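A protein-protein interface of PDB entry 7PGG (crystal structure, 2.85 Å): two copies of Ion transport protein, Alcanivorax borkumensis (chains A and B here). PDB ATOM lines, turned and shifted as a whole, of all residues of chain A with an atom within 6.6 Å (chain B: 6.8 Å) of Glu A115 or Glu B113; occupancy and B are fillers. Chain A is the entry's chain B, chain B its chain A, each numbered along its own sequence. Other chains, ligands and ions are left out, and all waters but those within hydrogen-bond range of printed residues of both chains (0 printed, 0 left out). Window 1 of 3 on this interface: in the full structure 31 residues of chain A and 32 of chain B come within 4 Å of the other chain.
The backbone carbonyl oxygen (O) of Glu B113 lies within hydrogen-bond range of the side-chain amide nitrogen (ND2) of Asn B117 (3.2 Å).
O of Arg A114 lies within hydrogen-bond range of ND2 of Asn A118, at 2.8 Å.
Printed residues of chain A that touch a printed residue of chain B: Arg A114, Glu A115 and Asn A118.
Of the 11 printed residues of chain B, 3 touch a printed residue of chain A.
Among the printed residues, merely in contact across the chains: Arg A114 with Gln B110 (3.7 Å), Asn A118 with Asn B117 (3.7 Å) and Glu A115 with Glu B113 (3.9 Å).
Arg A114 touches Gln B110, but with the chains exchanged Gln A110 does not touch Arg B114 (10.1 Å).
Glu A115 touches Glu B113, but with the chains exchanged Glu A113 does not touch Glu B115 (14.8 Å).
Asn A118 touches Asn B117, but with the chains exchanged Asn A117 does not touch Asn B118 (10.8 Å).
Positions printed for both chains: 110, 111, 112, 113, 114, 115, 116, 117 and 118.
Of the 3 pairs that touch across the chains among the printed residues, none has its exchanged pair printed and touching as well.
Glu A115 touches one residue of chain B.
Glu B113 touches just one residue of chain A: Glu A115 (3.9 Å).
Of the printed residues of chain A, Gln B110 touches Arg A114.
Of the printed residues of chain B, Arg A114 touches Gln B110 (3.7 Å).
Of the printed residues of chain A, Asn B117 touches Asn A118 (3.7 Å).
Arg B114 touches none of the printed residues of chain A.
Leu A119 touches none of the printed residues of chain B.
The nearest residue of chain B that does not touch Glu A115 is Asn B117 (6.0 Å).
The nearest residue of chain A that does not touch Glu B113 is Arg A111 (5.8 Å).
The nearest printed residue of chain A that does not touch Asn B117 is Glu A115 (6.0 Å).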
ATOM      1  N   GLN A 110      16.386  20.603   3.501  1.00  0.00           N
ATOM      2  CA  GLN A 110      17.658  20.929   4.142  1.00  0.00           C
ATOM      3  C   GLN A 110      17.628  20.613   5.637  1.00  0.00           C
ATOM      4  O   GLN A 110      18.616  20.113   6.186  1.00  0.00           O
ATOM      5  CB  GLN A 110      17.939  22.408   3.904  1.00  0.00           C
ATOM      6  CG  GLN A 110      18.208  22.869   2.456  1.00  0.00           C
ATOM      7  CD  GLN A 110      19.653  23.078   2.080  1.00  0.00           C
ATOM      8  OE1 GLN A 110      20.436  23.552   2.903  1.00  0.00           O
ATOM      9  NE2 GLN A 110      19.975  22.905   0.803  1.00  0.00           N
ATOM     10  N   ARG A 111      16.515  20.910   6.319  1.00  0.00           N
ATOM     11  CA  ARG A 111      16.367  20.453   7.698  1.00  0.00           C
ATOM     12  C   ARG A 111      16.335  18.931   7.772  1.00  0.00           C
ATOM     13  O   ARG A 111      16.856  18.338   8.725  1.00  0.00           O
ATOM     14  CB  ARG A 111      15.106  21.037   8.336  1.00  0.00           C
ATOM     15  CG  ARG A 111      15.173  22.523   8.635  1.00  0.00           C
ATOM     16  CD  ARG A 111      13.987  22.971   9.485  1.00  0.00           C
ATOM     17  NE  ARG A 111      12.717  22.829   8.780  1.00  0.00           N
ATOM     18  CZ  ARG A 111      12.184  23.776   8.016  1.00  0.00           C
ATOM     19  NH1 ARG A 111      12.806  24.938   7.870  1.00  0.00           N
ATOM     20  NH2 ARG A 111      11.026  23.567   7.402  1.00  0.00           N
ATOM     21  N   ALA A 112      15.715  18.284   6.782  1.00  0.00           N
ATOM     22  CA  ALA A 112      15.703  16.825   6.736  1.00  0.00           C
ATOM     23  C   ALA A 112      17.115  16.255   6.607  1.00  0.00           C
ATOM     24  O   ALA A 112      17.439  15.244   7.238  1.00  0.00           O
ATOM     25  CB  ALA A 112      14.826  16.347   5.582  1.00  0.00           C
ATOM     26  N   GLU A 113      17.965  16.878   5.779  1.00  0.00           N
ATOM     27  CA  GLU A 113      19.360  16.441   5.675  1.00  0.00           C
ATOM     28  C   GLU A 113      20.157  16.688   6.938  1.00  0.00           C
ATOM     29  O   GLU A 113      21.067  15.916   7.260  1.00  0.00           O
ATOM     30  CB  GLU A 113      20.087  17.106   4.509  1.00  0.00           C
ATOM     31  CG  GLU A 113      20.258  16.277   3.273  1.00  0.00           C
ATOM     32  CD  GLU A 113      20.947  17.040   2.163  1.00  0.00           C
ATOM     33  OE1 GLU A 113      21.014  18.282   2.253  1.00  0.00           O
ATOM     34  OE2 GLU A 113      21.472  16.397   1.229  1.00  0.00           O
ATOM     35  N   ARG A 114      19.872  17.772   7.638  1.00  0.00           N
ATOM     36  CA  ARG A 114      20.745  18.152   8.729  1.00  0.00           C
ATOM     37  C   ARG A 114      20.469  17.278   9.957  1.00  0.00           C
ATOM     38  O   ARG A 114      21.410  16.790  10.595  1.00  0.00           O
ATOM     39  CB  ARG A 114      20.565  19.658   8.934  1.00  0.00           C
ATOM     40  CG  ARG A 114      21.635  20.379   9.631  1.00  0.00           C
ATOM     41  CD  ARG A 114      21.575  21.889   9.516  1.00  0.00           C
ATOM     42  NE  ARG A 114      20.269  22.482   9.769  1.00  0.00           N
ATOM     43  CZ  ARG A 114      19.633  23.204   8.849  1.00  0.00           C
ATOM     44  NH1 ARG A 114      20.220  23.433   7.681  1.00  0.00           N
ATOM     45  NH2 ARG A 114      18.441  23.725   9.097  1.00  0.00           N
ATOM     46  N   GLU A 115      19.190  16.990  10.251  1.00  0.00           N
ATOM     47  CA  GLU A 115      18.912  15.991  11.278  1.00  0.00           C
ATOM     48  C   GLU A 115      19.161  14.564  10.804  1.00  0.00           C
ATOM     49  O   GLU A 115      19.288  13.662  11.641  1.00  0.00           O
ATOM     50  CB  GLU A 115      17.487  16.054  11.852  1.00  0.00           C
ATOM     51  CG  GLU A 115      17.119  17.257  12.737  1.00  0.00           C
ATOM     52  CD  GLU A 115      16.026  18.149  12.209  1.00  0.00           C
ATOM     53  OE1 GLU A 115      15.397  17.796  11.190  1.00  0.00           O
ATOM     54  OE2 GLU A 115      15.740  19.162  12.884  1.00  0.00           O
ATOM     55  N   ALA A 116      19.237  14.332   9.495  1.00  0.00           N
ATOM     56  CA  ALA A 116      19.672  13.025   9.021  1.00  0.00           C
ATOM     57  C   ALA A 116      21.126  12.776   9.391  1.00  0.00           C
ATOM     58  O   ALA A 116      21.483  11.683   9.846  1.00  0.00           O
ATOM     59  CB  ALA A 116      19.482  12.909   7.511  1.00  0.00           C
ATOM     60  N   ASN A 117      21.981  13.784   9.203  1.00  0.00           N
ATOM     61  CA  ASN A 117      23.385  13.649   9.574  1.00  0.00           C
ATOM     62  C   ASN A 117      23.571  13.717  11.084  1.00  0.00           C
ATOM     63  O   ASN A 117      24.381  12.972  11.647  1.00  0.00           O
ATOM     64  CB  ASN A 117      24.218  14.730   8.884  1.00  0.00           C
ATOM     65  CG  ASN A 117      24.339  14.507   7.392  1.00  0.00           C
ATOM     66  OD1 ASN A 117      24.538  13.381   6.938  1.00  0.00           O
ATOM     67  ND2 ASN A 117      24.223  15.582   6.620  1.00  0.00           N
ATOM     68  N   ASN A 118      22.841  14.611  11.759  1.00  0.00           N
ATOM     69  CA  ASN A 118      22.940  14.697  13.214  1.00  0.00           C
ATOM     70  C   ASN A 118      22.493  13.405  13.887  1.00  0.00           C
ATOM     71  O   ASN A 118      22.966  13.080  14.984  1.00  0.00           O
ATOM     72  CB  ASN A 118      22.121  15.881  13.731  1.00  0.00           C
ATOM     73  CG  ASN A 118      22.743  17.218  13.376  1.00  0.00           C
ATOM     74  OD1 ASN A 118      23.958  17.395  13.458  1.00  0.00           O
ATOM     75  ND2 ASN A 118      21.907  18.172  12.982  1.00  0.00           N
ATOM     76  N   LEU A 119      21.592  12.655  13.251  1.00  0.00           N
ATOM     77  CA  LEU A 119      21.225  11.342  13.770  1.00  0.00           C
ATOM     78  C   LEU A 119      22.363  10.343  13.589  1.00  0.00           C
ATOM     79  O   LEU A 119      22.712   9.608  14.521  1.00  0.00           O
ATOM     80  CB  LEU A 119      19.957  10.839  13.081  1.00  0.00           C
ATOM     81  CG  LEU A 119      19.434   9.491  13.579  1.00  0.00           C
ATOM     82  CD1 LEU A 119      19.032   9.572  15.047  1.00  0.00           C
ATOM     83  CD2 LEU A 119      18.277   8.998  12.723  1.00  0.00           C
ATOM     84  N   ILE A 120      22.943  10.293  12.388  1.00  0.00           N
ATOM     85  CA  ILE A 120      24.051   9.378  12.121  1.00  0.00           C
ATOM     86  C   ILE A 120      25.224   9.675  13.047  1.00  0.00           C
ATOM     87  O   ILE A 120      25.867   8.759  13.571  1.00  0.00           O
ATOM     88  CB  ILE A 120      24.465   9.460  10.639  1.00  0.00           C
ATOM     89  CG1 ILE A 120      23.284   9.099   9.740  1.00  0.00           C
ATOM     90  CG2 ILE A 120      25.643   8.543  10.365  1.00  0.00           C
ATOM     91  CD1 ILE A 120      22.756   7.696   9.955  1.00  0.00           C
ATOM     92  N   SER B 108      16.541  32.935  15.340  1.00  0.00           N
ATOM     93  CA  SER B 108      17.037  32.812  16.698  1.00  0.00           C
ATOM     94  C   SER B 108      16.883  31.362  17.168  1.00  0.00           C
ATOM     95  O   SER B 108      17.773  30.808  17.824  1.00  0.00           O
ATOM     96  CB  SER B 108      16.251  33.804  17.556  1.00  0.00           C
ATOM     97  OG  SER B 108      16.951  34.292  18.664  1.00  0.00           O
ATOM     98  N   GLU B 109      15.777  30.715  16.777  1.00  0.00           N
ATOM     99  CA  GLU B 109      15.562  29.306  17.098  1.00  0.00           C
ATOM    100  C   GLU B 109      16.582  28.406  16.413  1.00  0.00           C
ATOM    101  O   GLU B 109      16.870  27.307  16.908  1.00  0.00           O
ATOM    102  CB  GLU B 109      14.145  28.892  16.702  1.00  0.00           C
ATOM    103  CG  GLU B 109      13.046  29.569  17.509  1.00  0.00           C
ATOM    104  CD  GLU B 109      11.657  29.158  17.063  1.00  0.00           C
ATOM    105  OE1 GLU B 109      11.547  28.438  16.047  1.00  0.00           O
ATOM    106  OE2 GLU B 109      10.674  29.558  17.724  1.00  0.00           O
ATOM    107  N   GLN B 110      17.140  28.840  15.277  1.00  0.00           N
ATOM    108  CA  GLN B 110      18.062  27.957  14.575  1.00  0.00           C
ATOM    109  C   GLN B 110      19.467  28.014  15.149  1.00  0.00           C
ATOM    110  O   GLN B 110      20.160  26.990  15.179  1.00  0.00           O
ATOM    111  CB  GLN B 110      18.094  28.223  13.070  1.00  0.00           C
ATOM    112  CG  GLN B 110      16.739  27.937  12.495  1.00  0.00           C
ATOM    113  CD  GLN B 110      16.780  27.287  11.145  1.00  0.00           C
ATOM    114  OE1 GLN B 110      17.843  27.092  10.557  1.00  0.00           O
ATOM    115  NE2 GLN B 110      15.626  26.793  10.718  1.00  0.00           N
ATOM    116  N   ARG B 111      19.902  29.179  15.622  1.00  0.00           N
ATOM    117  CA  ARG B 111      21.137  29.212  16.397  1.00  0.00           C
ATOM    118  C   ARG B 111      20.993  28.423  17.692  1.00  0.00           C
ATOM    119  O   ARG B 111      21.942  27.770  18.138  1.00  0.00           O
ATOM    120  CB  ARG B 111      21.545  30.651  16.698  1.00  0.00           C
ATOM    121  CG  ARG B 111      22.045  31.429  15.494  1.00  0.00           C
ATOM    122  CD  ARG B 111      22.655  32.761  15.922  1.00  0.00           C
ATOM    123  NE  ARG B 111      21.664  33.655  16.515  1.00  0.00           N
ATOM    124  CZ  ARG B 111      20.932  34.518  15.819  1.00  0.00           C
ATOM    125  NH1 ARG B 111      21.088  34.609  14.505  1.00  0.00           N
ATOM    126  NH2 ARG B 111      20.048  35.292  16.432  1.00  0.00           N
ATOM    127  N   ALA B 112      19.817  28.490  18.319  1.00  0.00           N
ATOM    128  CA  ALA B 112      19.572  27.700  19.519  1.00  0.00           C
ATOM    129  C   ALA B 112      19.706  26.213  19.238  1.00  0.00           C
ATOM    130  O   ALA B 112      20.188  25.456  20.088  1.00  0.00           O
ATOM    131  CB  ALA B 112      18.188  28.013  20.078  1.00  0.00           C
ATOM    132  N   GLU B 113      19.341  25.786  18.035  1.00  0.00           N
ATOM    133  CA  GLU B 113      19.313  24.368  17.740  1.00  0.00           C
ATOM    134  C   GLU B 113      20.716  23.892  17.348  1.00  0.00           C
ATOM    135  O   GLU B 113      21.090  22.756  17.664  1.00  0.00           O
ATOM    136  CB  GLU B 113      18.282  24.144  16.631  1.00  0.00           C
ATOM    137  CG  GLU B 113      17.442  22.897  16.716  1.00  0.00           C
ATOM    138  CD  GLU B 113      16.452  22.787  15.565  1.00  0.00           C
ATOM    139  OE1 GLU B 113      16.560  23.587  14.613  1.00  0.00           O
ATOM    140  OE2 GLU B 113      15.541  21.933  15.631  1.00  0.00           O
ATOM    141  N   ARG B 114      21.520  24.755  16.696  1.00  0.00           N
ATOM    142  CA  ARG B 114      22.902  24.386  16.353  1.00  0.00           C
ATOM    143  C   ARG B 114      23.791  24.237  17.576  1.00  0.00           C
ATOM    144  O   ARG B 114      24.552  23.270  17.677  1.00  0.00           O
ATOM    145  CB  ARG B 114      23.570  25.375  15.394  1.00  0.00           C
ATOM    146  CG  ARG B 114      23.465  25.071  13.959  1.00  0.00           C
ATOM    147  CD  ARG B 114      24.387  25.883  13.077  1.00  0.00           C
ATOM    148  NE  ARG B 114      24.258  27.324  13.273  1.00  0.00           N
ATOM    149  CZ  ARG B 114      23.344  28.098  12.701  1.00  0.00           C
ATOM    150  NH1 ARG B 114      22.420  27.574  11.908  1.00  0.00           N
ATOM    151  NH2 ARG B 114      23.339  29.402  12.948  1.00  0.00           N
ATOM    152  N   GLU B 115      23.780  25.219  18.472  1.00  0.00           N
ATOM    153  CA  GLU B 115      24.552  25.103  19.705  1.00  0.00           C
ATOM    154  C   GLU B 115      23.964  24.066  20.646  1.00  0.00           C
ATOM    155  O   GLU B 115      24.677  23.563  21.517  1.00  0.00           O
ATOM    156  CB  GLU B 115      24.626  26.481  20.340  1.00  0.00           C
ATOM    157  CG  GLU B 115      25.558  27.388  19.568  1.00  0.00           C
ATOM    158  CD  GLU B 115      25.127  28.823  19.610  1.00  0.00           C
ATOM    159  OE1 GLU B 115      23.995  29.077  20.075  1.00  0.00           O
ATOM    160  OE2 GLU B 115      25.871  29.680  19.093  1.00  0.00           O
ATOM    161  N   ALA B 116      22.688  23.717  20.476  1.00  0.00           N
ATOM    162  CA  ALA B 116      22.143  22.582  21.210  1.00  0.00           C
ATOM    163  C   ALA B 116      22.802  21.285  20.764  1.00  0.00           C
ATOM    164  O   ALA B 116      23.178  20.449  21.593  1.00  0.00           O
ATOM    165  CB  ALA B 116      20.629  22.502  21.027  1.00  0.00           C
ATOM    166  N   ASN B 117      22.951  21.103  19.449  1.00  0.00           N
ATOM    167  CA  ASN B 117      23.609  19.905  18.936  1.00  0.00           C
ATOM    168  C   ASN B 117      25.117  19.968  19.143  1.00  0.00           C
ATOM    169  O   ASN B 117      25.742  18.957  19.483  1.00  0.00           O
ATOM    170  CB  ASN B 117      23.280  19.714  17.455  1.00  0.00           C
ATOM    171  CG  ASN B 117      21.839  19.309  17.226  1.00  0.00           C
ATOM    172  OD1 ASN B 117      21.294  18.481  17.956  1.00  0.00           O
ATOM    173  ND2 ASN B 117      21.212  19.894  16.211  1.00  0.00           N
ATOM    174  N   ASN B 118      25.723  21.141  18.934  1.00  0.00           N
ATOM    175  CA  ASN B 118      27.160  21.277  19.152  1.00  0.00           C
ATOM    176  C   ASN B 118      27.533  21.035  20.610  1.00  0.00           C
ATOM    177  O   ASN B 118      28.654  20.600  20.899  1.00  0.00           O
ATOM    178  CB  ASN B 118      27.634  22.659  18.703  1.00  0.00           C
ATOM    179  CG  ASN B 118      27.612  22.823  17.197  1.00  0.00           C
ATOM    180  OD1 ASN B 118      27.991  21.916  16.457  1.00  0.00           O
ATOM    181  ND2 ASN B 118      27.173  23.987  16.736  1.00  0.00           N
